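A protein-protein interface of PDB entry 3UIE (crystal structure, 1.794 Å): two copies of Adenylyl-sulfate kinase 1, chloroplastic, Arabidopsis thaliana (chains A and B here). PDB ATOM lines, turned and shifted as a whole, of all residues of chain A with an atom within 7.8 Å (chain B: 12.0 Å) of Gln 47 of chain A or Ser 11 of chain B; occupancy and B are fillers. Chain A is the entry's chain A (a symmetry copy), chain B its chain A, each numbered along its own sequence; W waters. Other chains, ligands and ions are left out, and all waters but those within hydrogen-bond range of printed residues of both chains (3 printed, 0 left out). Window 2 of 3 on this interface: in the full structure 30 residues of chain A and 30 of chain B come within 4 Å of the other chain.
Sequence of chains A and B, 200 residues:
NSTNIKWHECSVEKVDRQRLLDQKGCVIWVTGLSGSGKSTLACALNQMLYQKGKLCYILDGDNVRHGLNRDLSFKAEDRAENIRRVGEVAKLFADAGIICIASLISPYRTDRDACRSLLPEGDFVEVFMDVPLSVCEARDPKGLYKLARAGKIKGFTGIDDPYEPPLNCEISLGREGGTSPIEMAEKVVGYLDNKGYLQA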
ATOM      1  N   LEU A  41       7.767  -3.796 -10.165  1.00  0.00           N
ATOM      2  CA  LEU A  41       8.672  -2.957 -10.944  1.00  0.00           C
ATOM      3  C   LEU A  41       8.534  -3.240 -12.450  1.00  0.00           C
ATOM      4  O   LEU A  41       8.471  -2.314 -13.263  1.00  0.00           O
ATOM      5  CB  LEU A  41      10.115  -3.176 -10.505  1.00  0.00           C
ATOM      6  CG  LEU A  41      11.077  -2.489 -11.482  1.00  0.00           C
ATOM      7  CD1 LEU A  41      10.992  -0.974 -11.348  1.00  0.00           C
ATOM      8  CD2 LEU A  41      12.490  -2.990 -11.299  1.00  0.00           C
ATOM      9  N   ALA A  42       8.490  -4.512 -12.826  1.00  0.00           N
ATOM     10  CA  ALA A  42       8.345  -4.843 -14.246  1.00  0.00           C
ATOM     11  C   ALA A  42       7.095  -4.204 -14.867  1.00  0.00           C
ATOM     12  O   ALA A  42       7.151  -3.670 -15.962  1.00  0.00           O
ATOM     13  CB  ALA A  42       8.349  -6.360 -14.466  1.00  0.00           C
ATOM     14  N   CYS A  43       5.975  -4.281 -14.165  1.00  0.00           N
ATOM     15  CA  CYS A  43       4.740  -3.673 -14.643  1.00  0.00           C
ATOM     16  C   CYS A  43       4.882  -2.163 -14.764  1.00  0.00           C
ATOM     17  O   CYS A  43       4.570  -1.592 -15.805  1.00  0.00           O
ATOM     18  CB  CYS A  43       3.556  -4.029 -13.733  1.00  0.00           C
ATOM     19  SG  CYS A  43       3.022  -5.765 -13.821  1.00  0.00           S
ATOM     20  N   ALA A  44       5.359  -1.511 -13.702  1.00  0.00           N
ATOM     21  CA  ALA A  44       5.504  -0.057 -13.719  1.00  0.00           C
ATOM     22  C   ALA A  44       6.370   0.376 -14.904  1.00  0.00           C
ATOM     23  O   ALA A  44       6.042   1.333 -15.605  1.00  0.00           O
ATOM     24  CB  ALA A  44       6.100   0.459 -12.393  1.00  0.00           C
ATOM     25  N   LEU A  45       7.467  -0.342 -15.124  1.00  0.00           N
ATOM     26  CA  LEU A  45       8.373  -0.053 -16.229  1.00  0.00           C
ATOM     27  C   LEU A  45       7.677  -0.203 -17.584  1.00  0.00           C
ATOM     28  O   LEU A  45       7.774   0.665 -18.453  1.00  0.00           O
ATOM     29  CB  LEU A  45       9.603  -0.970 -16.142  1.00  0.00           C
ATOM     30  CG  LEU A  45      10.682  -0.898 -17.212  1.00  0.00           C
ATOM     31  CD1 LEU A  45      11.230   0.527 -17.346  1.00  0.00           C
ATOM     32  CD2 LEU A  45      11.806  -1.873 -16.861  1.00  0.00           C
ATOM     33  N   ASN A  46       6.960  -1.308 -17.755  1.00  0.00           N
ATOM     34  CA  ASN A  46       6.247  -1.581 -18.996  1.00  0.00           C
ATOM     35  C   ASN A  46       5.228  -0.476 -19.259  1.00  0.00           C
ATOM     36  O   ASN A  46       5.124   0.034 -20.368  1.00  0.00           O
ATOM     37  CB  ASN A  46       5.551  -2.930 -18.864  1.00  0.00           C
ATOM     38  CG  ASN A  46       4.945  -3.431 -20.175  1.00  0.00           C
ATOM     39  OD1 ASN A  46       5.190  -2.886 -21.242  1.00  0.00           O
ATOM     40  ND2 ASN A  46       4.157  -4.479 -20.077  1.00  0.00           N
ATOM     41  N   GLN A  47       4.500  -0.083 -18.222  1.00  0.00           N
ATOM     42  CA  GLN A  47       3.487   0.948 -18.383  1.00  0.00           C
ATOM     43  C   GLN A  47       4.117   2.256 -18.860  1.00  0.00           C
ATOM     44  O   GLN A  47       3.597   2.926 -19.750  1.00  0.00           O
ATOM     45  CB  GLN A  47       2.769   1.177 -17.056  1.00  0.00           C
ATOM     46  CG  GLN A  47       1.878   2.387 -17.062  1.00  0.00           C
ATOM     47  CD  GLN A  47       0.550   2.116 -17.731  1.00  0.00           C
ATOM     48  OE1 GLN A  47       0.297   1.010 -18.213  1.00  0.00           O
ATOM     49  NE2 GLN A  47      -0.312   3.127 -17.760  1.00  0.00           N
ATOM     50  N   MET A  48       5.242   2.608 -18.247  1.00  0.00           N
ATOM     51  CA  MET A  48       5.921   3.870 -18.523  1.00  0.00           C
ATOM     52  C   MET A  48       6.516   3.860 -19.935  1.00  0.00           C
ATOM     53  O   MET A  48       6.423   4.850 -20.669  1.00  0.00           O
ATOM     54  CB  MET A  48       7.016   4.087 -17.471  1.00  0.00           C
ATOM     55  CG  MET A  48       7.730   5.418 -17.529  1.00  0.00           C
ATOM     56  SD  MET A  48       8.785   5.601 -16.049  1.00  0.00           S
ATOM     57  CE  MET A  48       7.547   5.540 -14.771  1.00  0.00           C
ATOM     58  N   LEU A  49       7.112   2.739 -20.327  1.00  0.00           N
ATOM     59  CA  LEU A  49       7.714   2.648 -21.652  1.00  0.00           C
ATOM     60  C   LEU A  49       6.640   2.633 -22.734  1.00  0.00           C
ATOM     61  O   LEU A  49       6.782   3.271 -23.773  1.00  0.00           O
ATOM     62  CB  LEU A  49       8.590   1.400 -21.763  1.00  0.00           C
ATOM     63  CG  LEU A  49       9.903   1.519 -20.988  1.00  0.00           C
ATOM     64  CD1 LEU A  49      10.581   0.161 -20.884  1.00  0.00           C
ATOM     65  CD2 LEU A  49      10.823   2.554 -21.631  1.00  0.00           C
ATOM     66  N   TYR A  50       5.544   1.941 -22.457  1.00  0.00           N
ATOM     67  CA  TYR A  50       4.436   1.895 -23.417  1.00  0.00           C
ATOM     68  C   TYR A  50       3.913   3.305 -23.667  1.00  0.00           C
ATOM     69  O   TYR A  50       3.637   3.667 -24.794  1.00  0.00           O
ATOM     70  CB  TYR A  50       3.300   1.003 -22.924  1.00  0.00           C
ATOM     71  CG  TYR A  50       2.182   0.971 -23.942  1.00  0.00           C
ATOM     72  CD1 TYR A  50       2.228   0.088 -25.007  1.00  0.00           C
ATOM     73  CD2 TYR A  50       1.129   1.882 -23.876  1.00  0.00           C
ATOM     74  CE1 TYR A  50       1.222   0.072 -25.976  1.00  0.00           C
ATOM     75  CE2 TYR A  50       0.132   1.882 -24.833  1.00  0.00           C
ATOM     76  CZ  TYR A  50       0.183   0.974 -25.874  1.00  0.00           C
ATOM     77  OH  TYR A  50      -0.798   0.973 -26.831  1.00  0.00           O
ATOM     78  N   GLN A  51       3.796   4.116 -22.614  1.00  0.00           N
ATOM     79  CA  GLN A  51       3.271   5.473 -22.785  1.00  0.00           C
ATOM     80  C   GLN A  51       4.231   6.351 -23.623  1.00  0.00           C
ATOM     81  O   GLN A  51       3.806   7.277 -24.307  1.00  0.00           O
ATOM     82  CB  GLN A  51       2.943   6.117 -21.429  1.00  0.00           C
ATOM     83  CG  GLN A  51       2.512   7.576 -21.524  1.00  0.00           C
ATOM     84  CD  GLN A  51       1.754   8.054 -20.285  1.00  0.00           C
ATOM     85  OE1 GLN A  51       1.182   7.248 -19.546  1.00  0.00           O
ATOM     86  NE2 GLN A  51       1.735   9.370 -20.066  1.00  0.00           N
ATOM     87  N   LYS A  52       5.516   6.025 -23.591  1.00  0.00           N
ATOM     88  CA  LYS A  52       6.498   6.689 -24.449  1.00  0.00           C
ATOM     89  C   LYS A  52       6.552   6.088 -25.868  1.00  0.00           C
ATOM     90  O   LYS A  52       7.374   6.493 -26.699  1.00  0.00           O
ATOM     91  CB  LYS A  52       7.884   6.619 -23.801  1.00  0.00           C
ATOM     92  CG  LYS A  52       7.998   7.368 -22.459  1.00  0.00           C
ATOM     93  CD  LYS A  52       9.327   7.089 -21.757  1.00  0.00           C
ATOM     94  CE  LYS A  52      10.472   7.914 -22.350  1.00  0.00           C
ATOM     95  NZ  LYS A  52      10.265   9.386 -22.208  1.00  0.00           N
ATOM     96  N   GLY A  53       5.685   5.120 -26.139  1.00  0.00           N
ATOM     97  CA  GLY A  53       5.609   4.507 -27.457  1.00  0.00           C
ATOM     98  C   GLY A  53       6.649   3.425 -27.687  1.00  0.00           C
ATOM     99  O   GLY A  53       6.977   3.094 -28.822  1.00  0.00           O
ATOM    100  N   LYS A  54       7.178   2.858 -26.608  1.00  0.00           N
ATOM    101  CA  LYS A  54       8.167   1.787 -26.757  1.00  0.00           C
ATOM    102  C   LYS A  54       7.529   0.422 -26.469  1.00  0.00           C
ATOM    103  O   LYS A  54       6.683   0.297 -25.583  1.00  0.00           O
ATOM    104  CB  LYS A  54       9.365   2.028 -25.840  1.00  0.00           C
ATOM    105  CG  LYS A  54       9.927   3.451 -25.942  1.00  0.00           C
ATOM    106  CD  LYS A  54      10.454   3.733 -27.341  1.00  0.00           C
ATOM    107  CE  LYS A  54      10.561   5.220 -27.613  1.00  0.00           C
ATOM    108  NZ  LYS A  54      10.986   5.500 -29.015  1.00  0.00           N
ATOM    109  N   CYS A  56       7.593  -3.228 -25.061  1.00  0.00           N
ATOM    110  CA  CYS A  56       8.230  -4.090 -24.063  1.00  0.00           C
ATOM    111  C   CYS A  56       7.447  -5.382 -23.948  1.00  0.00           C
ATOM    112  O   CYS A  56       6.277  -5.432 -24.302  1.00  0.00           O
ATOM    113  CB  CYS A  56       8.224  -3.438 -22.677  1.00  0.00           C
ATOM    114  SG  CYS A  56       9.102  -1.906 -22.580  1.00  0.00           S
ATOM    115  N   ILE A  58       7.113  -8.645 -20.909  1.00  0.00           N
ATOM    116  CA  ILE A  58       7.580  -9.179 -19.634  1.00  0.00           C
ATOM    117  C   ILE A  58       7.577 -10.700 -19.623  1.00  0.00           C
ATOM    118  O   ILE A  58       6.553 -11.322 -19.887  1.00  0.00           O
ATOM    119  CB  ILE A  58       6.684  -8.687 -18.469  1.00  0.00           C
ATOM    120  CG1 ILE A  58       6.732  -7.162 -18.365  1.00  0.00           C
ATOM    121  CG2 ILE A  58       7.119  -9.309 -17.127  1.00  0.00           C
ATOM    122  CD1 ILE A  58       5.731  -6.586 -17.357  1.00  0.00           C
ATOM    123  N   ILE A 101      11.687  -7.596 -20.513  1.00  0.00           N
ATOM    124  CA  ILE A 101      11.874  -7.491 -19.074  1.00  0.00           C
ATOM    125  C   ILE A 101      11.687  -8.865 -18.449  1.00  0.00           C
ATOM    126  O   ILE A 101      10.596  -9.417 -18.492  1.00  0.00           O
ATOM    127  CB  ILE A 101      10.845  -6.532 -18.461  1.00  0.00           C
ATOM    128  CG1 ILE A 101      10.926  -5.161 -19.150  1.00  0.00           C
ATOM    129  CG2 ILE A 101      11.056  -6.419 -16.927  1.00  0.00           C
ATOM    130  CD1 ILE A 101       9.704  -4.287 -18.895  1.00  0.00           C
ATOM    131  N   ILE A 182       6.787   3.493  -9.190  1.00  0.00           N
ATOM    132  CA  ILE A 182       6.883   4.490 -10.255  1.00  0.00           C
ATOM    133  C   ILE A 182       8.231   5.203 -10.231  1.00  0.00           C
ATOM    134  O   ILE A 182       8.856   5.391 -11.277  1.00  0.00           O
ATOM    135  CB  ILE A 182       5.730   5.519 -10.206  1.00  0.00           C
ATOM    136  CG1 ILE A 182       4.410   4.858 -10.614  1.00  0.00           C
ATOM    137  CG2 ILE A 182       5.999   6.662 -11.161  1.00  0.00           C
ATOM    138  CD1 ILE A 182       3.220   5.810 -10.543  1.00  0.00           C
ATOM    139  N   ALA A 185      10.762   2.791 -11.611  1.00  0.00           N
ATOM    140  CA  ALA A 185      10.683   2.672 -13.060  1.00  0.00           C
ATOM    141  C   ALA A 185      11.276   3.908 -13.723  1.00  0.00           C
ATOM    142  O   ALA A 185      11.913   3.810 -14.771  1.00  0.00           O
ATOM    143  CB  ALA A 185       9.222   2.431 -13.520  1.00  0.00           C
ATOM    144  N   VAL A 189      14.024   3.899 -16.590  1.00  0.00           N
ATOM    145  CA  VAL A 189      13.765   4.501 -17.898  1.00  0.00           C
ATOM    146  C   VAL A 189      14.830   5.550 -18.207  1.00  0.00           C
ATOM    147  O   VAL A 189      15.339   5.626 -19.324  1.00  0.00           O
ATOM    148  CB  VAL A 189      12.360   5.139 -17.969  1.00  0.00           C
ATOM    149  CG1 VAL A 189      12.258   6.084 -19.169  1.00  0.00           C
ATOM    150  CG2 VAL A 189      11.288   4.048 -18.068  1.00  0.00           C
ATOM    151  N   CYS B  10      -0.254  -7.259 -15.536  1.00  0.00           N
ATOM    152  CA  CYS B  10       0.123  -5.870 -15.792  1.00  0.00           C
ATOM    153  C   CYS B  10      -0.899  -5.155 -16.680  1.00  0.00           C
ATOM    154  O   CYS B  10      -1.577  -5.783 -17.494  1.00  0.00           O
ATOM    155  CB  CYS B  10       1.515  -5.799 -16.424  1.00  0.00           C
ATOM    156  SG  CYS B  10       2.091  -4.114 -16.713  1.00  0.00           S
ATOM    157  N   SER B  11      -0.988  -3.838 -16.527  1.00  0.00           N
ATOM    158  CA  SER B  11      -2.001  -3.036 -17.205  1.00  0.00           C
ATOM    159  C   SER B  11      -1.859  -3.010 -18.728  1.00  0.00           C
ATOM    160  O   SER B  11      -2.841  -2.809 -19.433  1.00  0.00           O
ATOM    161  CB  SER B  11      -1.979  -1.606 -16.670  1.00  0.00           C
ATOM    162  OG  SER B  11      -0.677  -1.055 -16.793  1.00  0.00           O
ATOM    163  N   VAL B  12      -0.646  -3.190 -19.242  1.00  0.00           N
ATOM    164  CA  VAL B  12      -0.465  -3.187 -20.701  1.00  0.00           C
ATOM    165  C   VAL B  12      -0.902  -4.514 -21.310  1.00  0.00           C
ATOM    166  O   VAL B  12      -0.299  -5.553 -21.040  1.00  0.00           O
ATOM    167  CB  VAL B  12       0.999  -2.908 -21.077  1.00  0.00           C
ATOM    168  CG1 VAL B  12       1.167  -2.860 -22.588  1.00  0.00           C
ATOM    169  CG2 VAL B  12       1.446  -1.600 -20.460  1.00  0.00           C
ATOM    170  N   GLU B  13      -1.929  -4.463 -22.158  1.00  0.00           N
ATOM    171  CA  GLU B  13      -2.540  -5.669 -22.733  1.00  0.00           C
ATOM    172  C   GLU B  13      -2.040  -5.975 -24.140  1.00  0.00           C
ATOM    173  O   GLU B  13      -1.419  -5.140 -24.787  1.00  0.00           O
ATOM    174  CB  GLU B  13      -4.060  -5.507 -22.786  1.00  0.00           C
ATOM    175  CG  GLU B  13      -4.744  -5.372 -21.438  1.00  0.00           C
ATOM    176  CD  GLU B  13      -6.254  -5.261 -21.560  1.00  0.00           C
ATOM    177  OE1 GLU B  13      -6.815  -5.780 -22.546  1.00  0.00           O
ATOM    178  OE2 GLU B  13      -6.881  -4.652 -20.668  1.00  0.00           O
ATOM    179  N   LYS B  14      -2.341  -7.176 -24.628  1.00  0.00           N
ATOM    180  CA  LYS B  14      -2.015  -7.529 -26.003  1.00  0.00           C
ATOM    181  C   LYS B  14      -2.595  -6.515 -26.985  1.00  0.00           C
ATOM    182  O   LYS B  14      -1.920  -6.124 -27.944  1.00  0.00           O
ATOM    183  CB  LYS B  14      -2.516  -8.933 -26.328  1.00  0.00           C
ATOM    184  CG  LYS B  14      -2.234  -9.411 -27.745  1.00  0.00           C
ATOM    185  CD  LYS B  14      -2.740 -10.846 -27.864  1.00  0.00           C
ATOM    186  CE  LYS B  14      -2.929 -11.275 -29.305  1.00  0.00           C
ATOM    187  NZ  LYS B  14      -4.049 -12.252 -29.408  1.00  0.00           N
ATOM    188  N   VAL B  15      -3.829  -6.069 -26.743  1.00  0.00           N
ATOM    189  CA  VAL B  15      -4.460  -5.108 -27.649  1.00  0.00           C
ATOM    190  C   VAL B  15      -3.758  -3.762 -27.649  1.00  0.00           C
ATOM    191  O   VAL B  15      -3.799  -3.046 -28.651  1.00  0.00           O
ATOM    192  CB  VAL B  15      -5.965  -4.902 -27.378  1.00  0.00           C
ATOM    193  CG1 VAL B  15      -6.761  -6.097 -27.886  1.00  0.00           C
ATOM    194  CG2 VAL B  15      -6.221  -4.653 -25.890  1.00  0.00           C
ATOM    195  N   ASP B  16      -3.117  -3.410 -26.532  1.00  0.00           N
ATOM    196  CA  ASP B  16      -2.339  -2.179 -26.490  1.00  0.00           C
ATOM    197  C   ASP B  16      -1.087  -2.316 -27.352  1.00  0.00           C
ATOM    198  O   ASP B  16      -0.726  -1.401 -28.093  1.00  0.00           O
ATOM    199  CB  ASP B  16      -1.967  -1.796 -25.042  1.00  0.00           C
ATOM    200  CG  ASP B  16      -3.187  -1.553 -24.179  1.00  0.00           C
ATOM    201  OD1 ASP B  16      -4.063  -0.762 -24.594  1.00  0.00           O
ATOM    202  OD2 ASP B  16      -3.279  -2.173 -23.105  1.00  0.00           O
ATOM    203  N   ARG B  17      -0.414  -3.459 -27.263  1.00  0.00           N
ATOM    204  CA  ARG B  17       0.762  -3.679 -28.097  1.00  0.00           C
ATOM    205  C   ARG B  17       0.361  -3.725 -29.581  1.00  0.00           C
ATOM    206  O   ARG B  17       1.086  -3.246 -30.453  1.00  0.00           O
ATOM    207  CB  ARG B  17       1.486  -4.966 -27.678  1.00  0.00           C
ATOM    208  CG  ARG B  17       2.146  -4.866 -26.286  1.00  0.00           C
ATOM    209  CD  ARG B  17       2.871  -6.156 -25.896  1.00  0.00           C
ATOM    210  NE  ARG B  17       1.966  -7.254 -25.552  1.00  0.00           N
ATOM    211  CZ  ARG B  17       1.495  -7.451 -24.323  1.00  0.00           C
ATOM    212  NH1 ARG B  17       1.843  -6.609 -23.360  1.00  0.00           N
ATOM    213  NH2 ARG B  17       0.674  -8.470 -24.051  1.00  0.00           N
ATOM    214  N   GLN B  18      -0.809  -4.272 -29.859  1.00  0.00           N
ATOM    215  CA  GLN B  18      -1.260  -4.379 -31.252  1.00  0.00           C
ATOM    216  C   GLN B  18      -1.574  -2.991 -31.800  1.00  0.00           C
ATOM    217  O   GLN B  18      -1.239  -2.665 -32.937  1.00  0.00           O
ATOM    218  CB  GLN B  18      -2.453  -5.321 -31.337  1.00  0.00           C
ATOM    219  CG  GLN B  18      -1.990  -6.757 -31.185  1.00  0.00           C
ATOM    220  CD  GLN B  18      -3.089  -7.786 -31.285  1.00  0.00           C
ATOM    221  OE1 GLN B  18      -2.811  -8.984 -31.279  1.00  0.00           O
ATOM    222  NE2 GLN B  18      -4.344  -7.334 -31.355  1.00  0.00           N
ATOM    223  N   ARG B  19      -2.172  -2.160 -30.954  1.00  0.00           N
ATOM    224  CA  ARG B  19      -2.474  -0.783 -31.297  1.00  0.00           C
ATOM    225  C   ARG B  19      -1.193  -0.002 -31.617  1.00  0.00           C
ATOM    226  O   ARG B  19      -1.152   0.797 -32.548  1.00  0.00           O
ATOM    227  CB  ARG B  19      -3.208  -0.130 -30.127  1.00  0.00           C
ATOM    228  CG  ARG B  19      -3.867   1.187 -30.447  1.00  0.00           C
ATOM    229  CD  ARG B  19      -5.018   1.428 -29.484  1.00  0.00           C
ATOM    230  NE  ARG B  19      -4.619   1.227 -28.096  1.00  0.00           N
ATOM    231  CZ  ARG B  19      -4.028   2.158 -27.358  1.00  0.00           C
ATOM    232  NH1 ARG B  19      -3.765   3.345 -27.893  1.00  0.00           N
ATOM    233  NH2 ARG B  19      -3.695   1.905 -26.095  1.00  0.00           N
ATOM    234  N   LEU B  20      -0.149  -0.237 -30.836  1.00  0.00           N
ATOM    235  CA  LEU B  20       1.144   0.392 -31.075  1.00  0.00           C
ATOM    236  C   LEU B  20       1.744  -0.034 -32.429  1.00  0.00           C
ATOM    237  O   LEU B  20       2.245   0.806 -33.180  1.00  0.00           O
ATOM    238  CB  LEU B  20       2.102   0.058 -29.929  1.00  0.00           C
ATOM    239  CG  LEU B  20       3.481   0.697 -29.919  1.00  0.00           C
ATOM    240  CD1 LEU B  20       3.351   2.213 -30.035  1.00  0.00           C
ATOM    241  CD2 LEU B  20       4.194   0.327 -28.634  1.00  0.00           C
ATOM    242  N   ASP B  95       1.659 -12.951 -28.231  1.00  0.00           N
ATOM    243  CA  ASP B  95       1.089 -12.154 -27.155  1.00  0.00           C
ATOM    244  C   ASP B  95       1.749 -10.763 -27.117  1.00  0.00           C
ATOM    245  O   ASP B  95       1.121  -9.775 -26.729  1.00  0.00           O
ATOM    246  CB  ASP B  95       1.215 -12.885 -25.809  1.00  0.00           C
ATOM    247  CG  ASP B  95       0.491 -12.172 -24.685  1.00  0.00           C
ATOM    248  OD1 ASP B  95      -0.671 -11.770 -24.894  1.00  0.00           O
ATOM    249  OD2 ASP B  95       1.086 -12.023 -23.596  1.00  0.00           O
HETATM  250  O   HOH W   1       4.003  -4.401 -23.238  1.00  0.00           O
HETATM  251  O   HOH W   2      -2.488   1.775 -16.722  1.00  0.00           O
HETATM  252  O   HOH W   3       2.304  -6.436 -19.878  1.00  0.00           O
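O of Val 12 of chain B is in hydrogen-bond range of NH1 of Arg 17 of chain B, 3.3 Å away. O of Leu 49 of chain A is in hydrogen-bond range of N of Lys 54 of chain A, at 2.9 Å. The backbone NH of Glu 13 of chain B sits at hydrogen-bond distance from the side-chain carboxylate of Asp 16 of chain B, at 2.8 Å. The side-chain carboxylate (OD1) of Asp 16 of chain B lies within salt-bridge range of the guanidinium group (NH2) of Arg 19 of chain B, 3.1 Å away. The guanidinium group (NH2) of Arg 17 of chain B lies within salt-bridge range of the side-chain carboxylate (OD2) of Asp 95 of chain B (3.6 Å).
SG of Cys 10 of chain B touches ND2 of Asn 46 of chain A (3.96 Å). Asn 46 of chain A touches Val 12 of chain B (ND2 to CB, 3.7 Å). CG2 of Val 12 of chain B touches OE1 of Gln 47 of chain A, 3.6 Å away. Val 12 of chain B touches Tyr 50 of chain A. CE1 of Tyr 50 of chain A touches CD2 of Leu 20 of chain B (3.995 Å). CD1 of Leu 20 of chain B touches O of Gly 53 of chain A, at 3.9 Å. CD2 of Leu 20 of chain B touches O of Lys 54 of chain A, at 3.9 Å. O of Cys 56 of chain A touches CD of Arg 17 of chain B, at 3.8 Å.
OH of Tyr 50 of chain A lies within hydrogen-bond range of O of Asp 16 of chain B (2.7 Å). The side-chain hydroxyl (OG) of Ser 11 of chain B is in hydrogen-bond range of the side-chain amide oxygen (OE1) of Gln 47 of chain A. The guanidinium group (NH2) of Arg 19 of chain B sits at hydrogen-bond distance from the side-chain hydroxyl (OH) of Tyr 50 of chain A (3.1 Å). SG of Cys 10 of chain B lies close to O of Cys 43 of chain A, 3.7 Å away.
No position is printed for both chains. Of the 12 pairs that touch across the chains among the printed residues, none has its exchanged pair printed and touching as well.
No residue of chain B comes within 4 Å of Ala 44 of chain A. Gln 47 of chain A touches two residues of chain B. No residue of chain B comes within 4 Å of Met 48 of chain A. Lys 52 of chain A touches none of the printed residues of chain B. Printed residues of chain B within 4 Å of Gly 53 of chain A: Leu 20. Of the printed residues of chain B, Lys 54 of chain A touches Leu 20. Of the printed residues of chain B, Cys 56 of chain A touches Arg 17 (3.8 Å). Ile 58 of chain A touches none of the printed residues of chain B. Printed residues of chain A within 4 Å of Ser 11 of chain B: Gln 47 (2.7 Å). Printed residues of chain A within 4 Å of Val 12 of chain B: Asn 46 (3.7 Å), Gln 47 (3.6 Å) and Tyr 50 (3.96 Å). The nearest printed residue of chain B that does not touch Gln 47 of chain A is Cys 10 of chain B (4.9 Å). The nearest printed residue of chain B that does not touch Lys 54 of chain A is Arg 17 of chain B (6.9 Å).
Printed residues of chain B that touch a printed residue of chain A: Cys 10, Ser 11, Val 12, Asp 16, Arg 17, Arg 19 and Leu 20. Hydrophobic or aromatic side chains of chain B within 4 Å of the printed part of chain A: Val 12 and Leu 20. Among the printed residues, no Asp or Glu carboxylate lies within 4 Å of a Lys or Arg side-chain nitrogen of the other chain.
Water W3 lies within hydrogen-bond range of ND2 of Asn 46 of chain A and O of Val 12 of chain B. Water W1 lies within hydrogen-bond range of O of Cys 56 of chain A, OD1 of Asn 46 of chain A and NH1 of Arg 17 of chain B. Water W2 lies within hydrogen-bond range of the side-chain amide nitrogen of Gln 47 of chain A (2.8 Å) and the side-chain hydroxyl of Ser 11 of chain B (3.4 Å).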
